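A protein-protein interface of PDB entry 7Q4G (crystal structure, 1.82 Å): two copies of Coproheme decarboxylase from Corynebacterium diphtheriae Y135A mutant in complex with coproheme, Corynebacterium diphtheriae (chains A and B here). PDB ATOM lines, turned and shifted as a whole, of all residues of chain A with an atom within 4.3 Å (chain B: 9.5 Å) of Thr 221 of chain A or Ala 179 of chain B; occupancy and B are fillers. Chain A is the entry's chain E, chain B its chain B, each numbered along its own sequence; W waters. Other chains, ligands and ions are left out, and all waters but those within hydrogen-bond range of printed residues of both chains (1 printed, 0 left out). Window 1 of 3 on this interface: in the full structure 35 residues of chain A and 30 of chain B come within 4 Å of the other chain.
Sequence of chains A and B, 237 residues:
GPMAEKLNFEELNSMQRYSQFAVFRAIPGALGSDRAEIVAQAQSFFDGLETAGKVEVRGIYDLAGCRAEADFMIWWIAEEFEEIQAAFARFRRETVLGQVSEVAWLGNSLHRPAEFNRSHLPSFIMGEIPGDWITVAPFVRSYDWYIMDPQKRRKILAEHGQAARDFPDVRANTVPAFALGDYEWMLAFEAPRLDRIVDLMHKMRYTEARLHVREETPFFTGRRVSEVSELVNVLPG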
ATOM      1  N   LEU A  63      16.155  -4.176  -0.004  1.00  0.00           N
ATOM      2  CA  LEU A  63      15.941  -5.050   1.129  1.00  0.00           C
ATOM      3  C   LEU A  63      16.020  -4.367   2.494  1.00  0.00           C
ATOM      4  O   LEU A  63      16.089  -5.070   3.532  1.00  0.00           O
ATOM      5  CB  LEU A  63      17.006  -6.181   1.122  1.00  0.00           C
ATOM      6  CG  LEU A  63      17.101  -6.958  -0.222  1.00  0.00           C
ATOM      7  CD1 LEU A  63      18.209  -8.003  -0.065  1.00  0.00           C
ATOM      8  CD2 LEU A  63      15.799  -7.593  -0.651  1.00  0.00           C
ATOM      9  N   CYS A  66      14.853  -5.759   6.108  1.00  0.00           N
ATOM     10  CA  CYS A  66      14.474  -7.175   6.122  1.00  0.00           C
ATOM     11  C   CYS A  66      15.345  -7.937   7.127  1.00  0.00           C
ATOM     12  O   CYS A  66      14.824  -8.611   8.040  1.00  0.00           O
ATOM     13  CB  CYS A  66      14.581  -7.780   4.744  1.00  0.00           C
ATOM     14  SG  CYS A  66      14.573  -9.614   4.790  1.00  0.00           S
ATOM     15  N   ILE A 134       8.793  -8.951  -3.332  1.00  0.00           N
ATOM     16  CA  ILE A 134       9.352 -10.280  -3.578  1.00  0.00           C
ATOM     17  C   ILE A 134       9.890 -10.849  -2.289  1.00  0.00           C
ATOM     18  O   ILE A 134      10.343 -10.103  -1.407  1.00  0.00           O
ATOM     19  CB  ILE A 134      10.492 -10.251  -4.616  1.00  0.00           C
ATOM     20  CG1 ILE A 134      10.708 -11.616  -5.207  1.00  0.00           C
ATOM     21  CG2 ILE A 134      11.799  -9.781  -3.959  1.00  0.00           C
ATOM     22  CD1 ILE A 134      11.644 -11.620  -6.372  1.00  0.00           C
ATOM     23  N   THR A 135       9.800 -12.178  -2.172  1.00  0.00           N
ATOM     24  CA  THR A 135      10.496 -12.935  -1.134  1.00  0.00           C
ATOM     25  C   THR A 135      11.271 -14.014  -1.843  1.00  0.00           C
ATOM     26  O   THR A 135      10.707 -14.719  -2.693  1.00  0.00           O
ATOM     27  CB  THR A 135       9.536 -13.559  -0.115  1.00  0.00           C
ATOM     28  OG1 THR A 135       8.954 -12.539   0.689  1.00  0.00           O
ATOM     29  CG2 THR A 135      10.267 -14.546   0.765  1.00  0.00           C
ATOM     30  N   LEU A 194       3.067  -6.854   0.108  1.00  0.00           N
ATOM     31  CA  LEU A 194       3.855  -7.758   0.944  1.00  0.00           C
ATOM     32  C   LEU A 194       2.949  -8.693   1.745  1.00  0.00           C
ATOM     33  O   LEU A 194       3.267  -9.864   1.954  1.00  0.00           O
ATOM     34  CB  LEU A 194       4.740  -6.925   1.888  1.00  0.00           C
ATOM     35  CG  LEU A 194       5.678  -7.786   2.757  1.00  0.00           C
ATOM     36  CD1 LEU A 194       6.525  -8.691   1.950  1.00  0.00           C
ATOM     37  CD2 LEU A 194       6.522  -6.823   3.606  1.00  0.00           C
ATOM     38  N   ILE A 197       2.196 -12.170   0.446  1.00  0.00           N
ATOM     39  CA  ILE A 197       3.245 -13.179   0.551  1.00  0.00           C
ATOM     40  C   ILE A 197       3.308 -13.771   1.957  1.00  0.00           C
ATOM     41  O   ILE A 197       3.481 -14.984   2.142  1.00  0.00           O
ATOM     42  CB  ILE A 197       4.613 -12.604   0.167  1.00  0.00           C
ATOM     43  CG1 ILE A 197       4.652 -12.206  -1.306  1.00  0.00           C
ATOM     44  CG2 ILE A 197       5.693 -13.670   0.455  1.00  0.00           C
ATOM     45  CD1 ILE A 197       5.857 -11.332  -1.619  1.00  0.00           C
ATOM     46  N   MET A 201       2.544 -17.879   2.828  1.00  0.00           N
ATOM     47  CA  MET A 201       3.466 -18.797   3.570  1.00  0.00           C
ATOM     48  C   MET A 201       2.790 -19.381   4.807  1.00  0.00           C
ATOM     49  O   MET A 201       2.941 -20.579   5.098  1.00  0.00           O
ATOM     50  CB  MET A 201       4.702 -18.080   3.979  1.00  0.00           C
ATOM     51  CG  MET A 201       5.417 -17.373   2.911  1.00  0.00           C
ATOM     52  SD  MET A 201       6.353 -18.507   1.947  1.00  0.00           S
ATOM     53  CE  MET A 201       7.783 -17.493   1.563  1.00  0.00           C
ATOM     54  N   PHE A 219      15.900 -16.071   4.224  1.00  0.00           N
ATOM     55  CA  PHE A 219      14.888 -15.349   3.461  1.00  0.00           C
ATOM     56  C   PHE A 219      15.377 -13.951   3.152  1.00  0.00           C
ATOM     57  O   PHE A 219      15.930 -13.277   4.022  1.00  0.00           O
ATOM     58  CB  PHE A 219      13.557 -15.257   4.249  1.00  0.00           C
ATOM     59  CG  PHE A 219      12.720 -16.500   4.165  1.00  0.00           C
ATOM     60  CD1 PHE A 219      12.985 -17.588   5.009  1.00  0.00           C
ATOM     61  CD2 PHE A 219      11.674 -16.604   3.254  1.00  0.00           C
ATOM     62  CE1 PHE A 219      12.206 -18.715   4.941  1.00  0.00           C
ATOM     63  CE2 PHE A 219      10.905 -17.760   3.172  1.00  0.00           C
ATOM     64  CZ  PHE A 219      11.190 -18.821   4.028  1.00  0.00           C
ATOM     65  N   PHE A 220      15.074 -13.484   1.939  1.00  0.00           N
ATOM     66  CA  PHE A 220      15.348 -12.109   1.524  1.00  0.00           C
ATOM     67  C   PHE A 220      14.083 -11.508   0.951  1.00  0.00           C
ATOM     68  O   PHE A 220      13.558 -12.015  -0.050  1.00  0.00           O
ATOM     69  CB  PHE A 220      16.488 -12.025   0.502  1.00  0.00           C
ATOM     70  CG  PHE A 220      17.742 -12.696   0.975  1.00  0.00           C
ATOM     71  CD1 PHE A 220      18.632 -12.012   1.745  1.00  0.00           C
ATOM     72  CD2 PHE A 220      17.955 -14.013   0.688  1.00  0.00           C
ATOM     73  CE1 PHE A 220      19.797 -12.657   2.231  1.00  0.00           C
ATOM     74  CE2 PHE A 220      19.080 -14.656   1.163  1.00  0.00           C
ATOM     75  CZ  PHE A 220      20.010 -13.971   1.902  1.00  0.00           C
ATOM     76  N   THR A 221      13.630 -10.411   1.558  1.00  0.00           N
ATOM     77  CA  THR A 221      12.358  -9.790   1.189  1.00  0.00           C
ATOM     78  C   THR A 221      12.560  -8.313   0.972  1.00  0.00           C
ATOM     79  O   THR A 221      13.253  -7.662   1.766  1.00  0.00           O
ATOM     80  CB  THR A 221      11.318 -10.019   2.277  1.00  0.00           C
ATOM     81  OG1 THR A 221      11.035 -11.415   2.314  1.00  0.00           O
ATOM     82  CG2 THR A 221      10.068  -9.282   2.004  1.00  0.00           C
ATOM     83  N   GLY A 222      11.934  -7.781  -0.105  1.00  0.00           N
ATOM     84  CA  GLY A 222      12.211  -6.400  -0.470  1.00  0.00           C
ATOM     85  C   GLY A 222      11.261  -5.883  -1.542  1.00  0.00           C
ATOM     86  O   GLY A 222      10.418  -6.613  -2.102  1.00  0.00           O
ATOM     87  N   TYR B  18       2.404  -3.559  10.548  1.00  0.00           N
ATOM     88  CA  TYR B  18       3.694  -4.210  10.575  1.00  0.00           C
ATOM     89  C   TYR B  18       4.428  -3.749  11.841  1.00  0.00           C
ATOM     90  O   TYR B  18       4.355  -2.610  12.260  1.00  0.00           O
ATOM     91  CB  TYR B  18       4.510  -3.872   9.333  1.00  0.00           C
ATOM     92  CG  TYR B  18       4.073  -4.546   8.056  1.00  0.00           C
ATOM     93  CD1 TYR B  18       4.594  -5.777   7.711  1.00  0.00           C
ATOM     94  CD2 TYR B  18       3.131  -3.980   7.213  1.00  0.00           C
ATOM     95  CE1 TYR B  18       4.169  -6.421   6.510  1.00  0.00           C
ATOM     96  CE2 TYR B  18       2.692  -4.613   6.072  1.00  0.00           C
ATOM     97  CZ  TYR B  18       3.238  -5.829   5.704  1.00  0.00           C
ATOM     98  OH  TYR B  18       2.821  -6.467   4.546  1.00  0.00           O
ATOM     99  N   GLN B  20       8.355  -3.962  13.860  1.00  0.00           N
ATOM    100  CA  GLN B  20       9.748  -4.273  13.699  1.00  0.00           C
ATOM    101  C   GLN B  20      10.476  -3.982  14.989  1.00  0.00           C
ATOM    102  O   GLN B  20      10.299  -2.904  15.569  1.00  0.00           O
ATOM    103  CB  GLN B  20      10.415  -3.457  12.553  1.00  0.00           C
ATOM    104  CG  GLN B  20      11.954  -3.603  12.562  1.00  0.00           C
ATOM    105  CD  GLN B  20      12.603  -2.903  11.380  1.00  0.00           C
ATOM    106  OE1 GLN B  20      13.020  -1.777  11.493  1.00  0.00           O
ATOM    107  NE2 GLN B  20      12.739  -3.608  10.264  1.00  0.00           N
ATOM    108  N   PHE B  81       4.817  -1.599   5.466  1.00  0.00           N
ATOM    109  CA  PHE B  81       6.199  -1.955   5.740  1.00  0.00           C
ATOM    110  C   PHE B  81       7.180  -1.001   5.078  1.00  0.00           C
ATOM    111  O   PHE B  81       8.212  -0.666   5.673  1.00  0.00           O
ATOM    112  CB  PHE B  81       6.483  -3.382   5.302  1.00  0.00           C
ATOM    113  CG  PHE B  81       7.832  -3.870   5.707  1.00  0.00           C
ATOM    114  CD1 PHE B  81       8.115  -4.160   7.055  1.00  0.00           C
ATOM    115  CD2 PHE B  81       8.843  -4.035   4.758  1.00  0.00           C
ATOM    116  CE1 PHE B  81       9.349  -4.593   7.439  1.00  0.00           C
ATOM    117  CE2 PHE B  81      10.097  -4.471   5.162  1.00  0.00           C
ATOM    118  CZ  PHE B  81      10.350  -4.753   6.482  1.00  0.00           C
ATOM    119  N   GLN B  85      10.645   0.624   6.378  1.00  0.00           N
ATOM    120  CA  GLN B  85      11.873   0.590   5.587  1.00  0.00           C
ATOM    121  C   GLN B  85      12.479   1.974   5.547  1.00  0.00           C
ATOM    122  O   GLN B  85      13.654   2.151   5.841  1.00  0.00           O
ATOM    123  CB  GLN B  85      11.607   0.090   4.165  1.00  0.00           C
ATOM    124  CG  GLN B  85      11.197  -1.375   4.062  1.00  0.00           C
ATOM    125  CD  GLN B  85      11.336  -1.904   2.638  1.00  0.00           C
ATOM    126  OE1 GLN B  85      10.447  -1.731   1.820  1.00  0.00           O
ATOM    127  NE2 GLN B  85      12.431  -2.583   2.350  1.00  0.00           N
ATOM    128  N   LEU B 106      17.069  -7.974  13.134  1.00  0.00           N
ATOM    129  CA  LEU B 106      15.801  -7.381  12.794  1.00  0.00           C
ATOM    130  C   LEU B 106      14.705  -8.423  12.947  1.00  0.00           C
ATOM    131  O   LEU B 106      14.746  -9.469  12.302  1.00  0.00           O
ATOM    132  CB  LEU B 106      15.839  -6.808  11.387  1.00  0.00           C
ATOM    133  CG  LEU B 106      16.817  -5.668  11.145  1.00  0.00           C
ATOM    134  CD1 LEU B 106      16.835  -5.230   9.680  1.00  0.00           C
ATOM    135  CD2 LEU B 106      16.489  -4.452  12.042  1.00  0.00           C
ATOM    136  N   ASN B 108      10.848  -8.788  12.250  1.00  0.00           N
ATOM    137  CA  ASN B 108       9.708  -8.208  11.549  1.00  0.00           C
ATOM    138  C   ASN B 108       8.485  -9.092  11.686  1.00  0.00           C
ATOM    139  O   ASN B 108       8.597 -10.333  11.726  1.00  0.00           O
ATOM    140  CB  ASN B 108      10.007  -8.003  10.068  1.00  0.00           C
ATOM    141  CG  ASN B 108      11.225  -7.101   9.855  1.00  0.00           C
ATOM    142  OD1 ASN B 108      11.343  -6.025  10.474  1.00  0.00           O
ATOM    143  ND2 ASN B 108      12.126  -7.516   8.995  1.00  0.00           N
ATOM    144  N   SER B 109       7.314  -8.460  11.701  1.00  0.00           N
ATOM    145  CA  SER B 109       6.060  -9.196  11.839  1.00  0.00           C
ATOM    146  C   SER B 109       4.868  -8.394  11.319  1.00  0.00           C
ATOM    147  O   SER B 109       4.913  -7.193  11.166  1.00  0.00           O
ATOM    148  CB  SER B 109       5.824  -9.612  13.275  1.00  0.00           C
ATOM    149  OG  SER B 109       5.773  -8.474  14.115  1.00  0.00           O
ATOM    150  N   LEU B 110       3.775  -9.110  11.091  1.00  0.00           N
ATOM    151  CA  LEU B 110       2.562  -8.545  10.544  1.00  0.00           C
ATOM    152  C   LEU B 110       1.386  -9.121  11.320  1.00  0.00           C
ATOM    153  O   LEU B 110       1.186 -10.341  11.333  1.00  0.00           O
ATOM    154  CB  LEU B 110       2.448  -8.875   9.074  1.00  0.00           C
ATOM    155  CG  LEU B 110       1.119  -8.469   8.413  1.00  0.00           C
ATOM    156  CD1 LEU B 110       0.864  -6.990   8.511  1.00  0.00           C
ATOM    157  CD2 LEU B 110       1.136  -8.950   6.923  1.00  0.00           C
ATOM    158  N   VAL B 175       2.985 -12.477  16.933  1.00  0.00           N
ATOM    159  CA  VAL B 175       2.708 -11.866  15.615  1.00  0.00           C
ATOM    160  C   VAL B 175       3.380 -12.683  14.498  1.00  0.00           C
ATOM    161  O   VAL B 175       4.555 -12.972  14.595  1.00  0.00           O
ATOM    162  CB  VAL B 175       3.183 -10.395  15.577  1.00  0.00           C
ATOM    163  CG1 VAL B 175       2.512  -9.627  14.511  1.00  0.00           C
ATOM    164  CG2 VAL B 175       2.952  -9.740  16.952  1.00  0.00           C
ATOM    165  N   PRO B 176       2.646 -13.069  13.453  1.00  0.00           N
ATOM    166  CA  PRO B 176       3.253 -13.767  12.321  1.00  0.00           C
ATOM    167  C   PRO B 176       4.459 -13.044  11.755  1.00  0.00           C
ATOM    168  O   PRO B 176       4.468 -11.828  11.597  1.00  0.00           O
ATOM    169  CB  PRO B 176       2.125 -13.861  11.265  1.00  0.00           C
ATOM    170  CG  PRO B 176       0.859 -13.712  12.057  1.00  0.00           C
ATOM    171  CD  PRO B 176       1.174 -12.984  13.341  1.00  0.00           C
ATOM    172  N   ALA B 177       5.500 -13.831  11.458  1.00  0.00           N
ATOM    173  CA  ALA B 177       6.723 -13.293  10.861  1.00  0.00           C
ATOM    174  C   ALA B 177       7.105 -14.003   9.576  1.00  0.00           C
ATOM    175  O   ALA B 177       8.175 -13.714   8.987  1.00  0.00           O
ATOM    176  CB  ALA B 177       7.852 -13.334  11.908  1.00  0.00           C
ATOM    177  N   PHE B 178       6.248 -14.896   9.095  1.00  0.00           N
ATOM    178  CA  PHE B 178       6.508 -15.643   7.854  1.00  0.00           C
ATOM    179  C   PHE B 178       6.959 -14.734   6.743  1.00  0.00           C
ATOM    180  O   PHE B 178       6.325 -13.740   6.464  1.00  0.00           O
ATOM    181  CB  PHE B 178       5.217 -16.360   7.404  1.00  0.00           C
ATOM    182  CG  PHE B 178       4.629 -17.256   8.476  1.00  0.00           C
ATOM    183  CD1 PHE B 178       5.103 -18.550   8.636  1.00  0.00           C
ATOM    184  CD2 PHE B 178       3.617 -16.810   9.304  1.00  0.00           C
ATOM    185  CE1 PHE B 178       4.555 -19.391   9.633  1.00  0.00           C
ATOM    186  CE2 PHE B 178       3.045 -17.625  10.260  1.00  0.00           C
ATOM    187  CZ  PHE B 178       3.532 -18.953  10.399  1.00  0.00           C
ATOM    188  N   ALA B 179       8.048 -15.124   6.053  1.00  0.00           N
ATOM    189  CA  ALA B 179       8.550 -14.375   4.894  1.00  0.00           C
ATOM    190  C   ALA B 179       9.148 -12.985   5.229  1.00  0.00           C
ATOM    191  O   ALA B 179       9.610 -12.273   4.302  1.00  0.00           O
ATOM    192  CB  ALA B 179       7.445 -14.105   3.841  1.00  0.00           C
ATOM    193  N   LEU B 180       9.113 -12.537   6.465  1.00  0.00           N
ATOM    194  CA  LEU B 180       9.715 -11.255   6.835  1.00  0.00           C
ATOM    195  C   LEU B 180      11.091 -11.452   7.520  1.00  0.00           C
ATOM    196  O   LEU B 180      11.520 -10.625   8.370  1.00  0.00           O
ATOM    197  CB  LEU B 180       8.783 -10.478   7.746  1.00  0.00           C
ATOM    198  CG  LEU B 180       7.359 -10.338   7.243  1.00  0.00           C
ATOM    199  CD1 LEU B 180       6.512  -9.617   8.281  1.00  0.00           C
ATOM    200  CD2 LEU B 180       7.382  -9.586   5.941  1.00  0.00           C
ATOM    201  N   GLY B 181      11.763 -12.537   7.195  1.00  0.00           N
ATOM    202  CA  GLY B 181      12.978 -12.962   7.859  1.00  0.00           C
ATOM    203  C   GLY B 181      12.986 -14.471   7.921  1.00  0.00           C
ATOM    204  O   GLY B 181      12.242 -15.112   7.218  1.00  0.00           O
ATOM    205  N   ASP B 182      13.743 -14.998   8.874  1.00  0.00           N
ATOM    206  CA  ASP B 182      13.956 -16.445   8.960  1.00  0.00           C
ATOM    207  C   ASP B 182      12.993 -17.167   9.900  1.00  0.00           C
ATOM    208  O   ASP B 182      13.203 -18.384  10.207  1.00  0.00           O
ATOM    209  CB  ASP B 182      15.390 -16.723   9.410  1.00  0.00           C
ATOM    210  CG  ASP B 182      16.406 -16.416   8.350  1.00  0.00           C
ATOM    211  OD1 ASP B 182      16.021 -16.266   7.157  1.00  0.00           O
ATOM    212  OD2 ASP B 182      17.588 -16.277   8.720  1.00  0.00           O
ATOM    213  N   TYR B 183      11.969 -16.505  10.374  1.00  0.00           N
ATOM    214  CA  TYR B 183      11.161 -17.074  11.467  1.00  0.00           C
ATOM    215  C   TYR B 183       9.688 -17.197  11.072  1.00  0.00           C
ATOM    216  O   TYR B 183       9.222 -16.737  10.024  1.00  0.00           O
ATOM    217  CB  TYR B 183      11.357 -16.217  12.737  1.00  0.00           C
ATOM    218  CG  TYR B 183      12.809 -15.936  13.001  1.00  0.00           C
ATOM    219  CD1 TYR B 183      13.693 -16.955  13.407  1.00  0.00           C
ATOM    220  CD2 TYR B 183      13.340 -14.678  12.811  1.00  0.00           C
ATOM    221  CE1 TYR B 183      15.045 -16.699  13.662  1.00  0.00           C
ATOM    222  CE2 TYR B 183      14.696 -14.391  13.068  1.00  0.00           C
ATOM    223  CZ  TYR B 183      15.550 -15.427  13.499  1.00  0.00           C
ATOM    224  OH  TYR B 183      16.867 -15.160  13.743  1.00  0.00           O
ATOM    225  N   GLU B 184       8.905 -17.788  11.979  1.00  0.00           N
ATOM    226  CA  GLU B 184       7.475 -17.923  11.795  1.00  0.00           C
ATOM    227  C   GLU B 184       6.664 -16.923  12.627  1.00  0.00           C
ATOM    228  O   GLU B 184       5.595 -16.499  12.187  1.00  0.00           O
ATOM    229  CB  GLU B 184       7.040 -19.328  12.143  1.00  0.00           C
ATOM    230  CG  GLU B 184       7.687 -20.377  11.256  1.00  0.00           C
ATOM    231  CD  GLU B 184       7.224 -21.790  11.566  1.00  0.00           C
ATOM    232  OE1 GLU B 184       6.663 -22.060  12.684  1.00  0.00           O
ATOM    233  OE2 GLU B 184       7.432 -22.664  10.668  1.00  0.00           O
ATOM    234  N   TRP B 185       7.164 -16.548  13.800  1.00  0.00           N
ATOM    235  CA  TRP B 185       6.511 -15.625  14.706  1.00  0.00           C
ATOM    236  C   TRP B 185       7.540 -14.680  15.326  1.00  0.00           C
ATOM    237  O   TRP B 185       8.726 -15.031  15.451  1.00  0.00           O
ATOM    238  CB  TRP B 185       5.787 -16.397  15.853  1.00  0.00           C
ATOM    239  CG  TRP B 185       4.796 -17.345  15.325  1.00  0.00           C
ATOM    240  CD1 TRP B 185       5.015 -18.675  14.974  1.00  0.00           C
ATOM    241  CD2 TRP B 185       3.445 -17.078  15.026  1.00  0.00           C
ATOM    242  NE1 TRP B 185       3.872 -19.221  14.507  1.00  0.00           N
ATOM    243  CE2 TRP B 185       2.881 -18.276  14.520  1.00  0.00           C
ATOM    244  CE3 TRP B 185       2.607 -15.950  15.167  1.00  0.00           C
ATOM    245  CZ2 TRP B 185       1.542 -18.359  14.098  1.00  0.00           C
ATOM    246  CZ3 TRP B 185       1.291 -16.053  14.741  1.00  0.00           C
ATOM    247  CH2 TRP B 185       0.752 -17.245  14.229  1.00  0.00           C
ATOM    248  N   MET B 186       7.067 -13.474  15.701  1.00  0.00           N
ATOM    249  CA  MET B 186       7.782 -12.537  16.577  1.00  0.00           C
ATOM    250  C   MET B 186       7.087 -12.528  17.936  1.00  0.00           C
ATOM    251  O   MET B 186       5.858 -12.496  18.021  1.00  0.00           O
ATOM    252  CB  MET B 186       7.789 -11.109  16.027  1.00  0.00           C
ATOM    253  CG  MET B 186       8.924 -10.817  15.058  1.00  0.00           C
ATOM    254  SD  MET B 186      10.607 -11.217  15.649  1.00  0.00           S
ATOM    255  CE  MET B 186      11.195 -12.237  14.365  1.00  0.00           C
HETATM  256  O   HOH W   1      15.573 -10.376   9.973  1.00  0.00           O
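Leu 106 of chain B touches Cys 66 of chain A (CB to O, 3.9 Å).
Cys 66 of chain A touches Leu 180 of chain B (O to O, 3.9 Å).
O of Ala 179 of chain B touches OG1 of Thr 135 of chain A, at 3.7 Å.
Tyr 18 of chain B touches Leu 194 of chain A (OH to CB, 3.3 Å).
Leu 194 of chain A touches Phe 81 of chain B (CD2 to CD2, 3.8 Å).
Leu 194 of chain A touches Leu 180 of chain B.
Ile 197 of chain A touches Ala 179 of chain B.
Met 201 of chain A touches Phe 178 of chain B.
Ala 179 of chain B touches Met 201 of chain A.
Gly 181 of chain B touches Phe 219 of chain A.
Of chain B, only Ala 179 (2.6 Å) comes within 4 Å of Thr 221 of chain A.
Of the printed residues of chain A, Ala 179 of chain B touches Thr 135 (3.7 Å), Ile 197 (3.8 Å), Met 201 (3.96 Å) and Thr 221 (2.6 Å).
Printed residues of chain B within 4 Å of Cys 66 of chain A: Leu 106, Asn 108 and Leu 180.
Printed residues of chain A within 4 Å of Leu 180 of chain B: Cys 66 and Leu 194.
The nearest printed residue of chain A that does not touch Ala 179 of chain B is Phe 219 of chain A (4.2 Å).
The side-chain carboxylate (OD1) of Asp 182 of chain B sits at hydrogen-bond distance from the backbone NH (N) of Phe 219 of chain A, 2.9 Å away.
ND2 of Asn 108 of chain B is in hydrogen-bond range of O of Cys 66 of chain A (3.1 Å).
The backbone carbonyl oxygen (O) of Ala 179 of chain B sits at hydrogen-bond distance from the side-chain hydroxyl (OG1) of Thr 221 of chain A (2.6 Å).
Printed residues of chain B that touch a printed residue of chain A: Tyr 18, Phe 81, Leu 106, Asn 108, Phe 178, Ala 179, Leu 180, Gly 181 and Asp 182.
Among the printed residues, no Asp or Glu carboxylate lies within 4 Å of a Lys or Arg side-chain nitrogen of the other chain.
Water W1 lies within hydrogen-bond range of the backbone carbonyl oxygen of Leu 106 of chain B and the backbone carbonyl oxygen of Cys 66 of chain A.
No position is printed for both chains.
Of the 13 pairs that touch across the chains among the printed residues, none has its exchanged pair printed and touching as well.
The side-chain hydroxyl (OG1) of Thr 135 of chain A lies within hydrogen-bond range of the side-chain hydroxyl (OG1) of Thr 221 of chain A, at 2.9 Å.
The side-chain amide nitrogen of Gln 20 of chain B lies within hydrogen-bond range of the side-chain amide oxygen of Asn 108 of chain B, at 2.8 Å.
N of Thr 221 of chain A sits at hydrogen-bond distance from SG of Cys 66 of chain A.
The side-chain amide nitrogen (ND2) of Asn 108 of chain B is in hydrogen-bond range of the backbone carbonyl oxygen (O) of Leu 180 of chain B.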
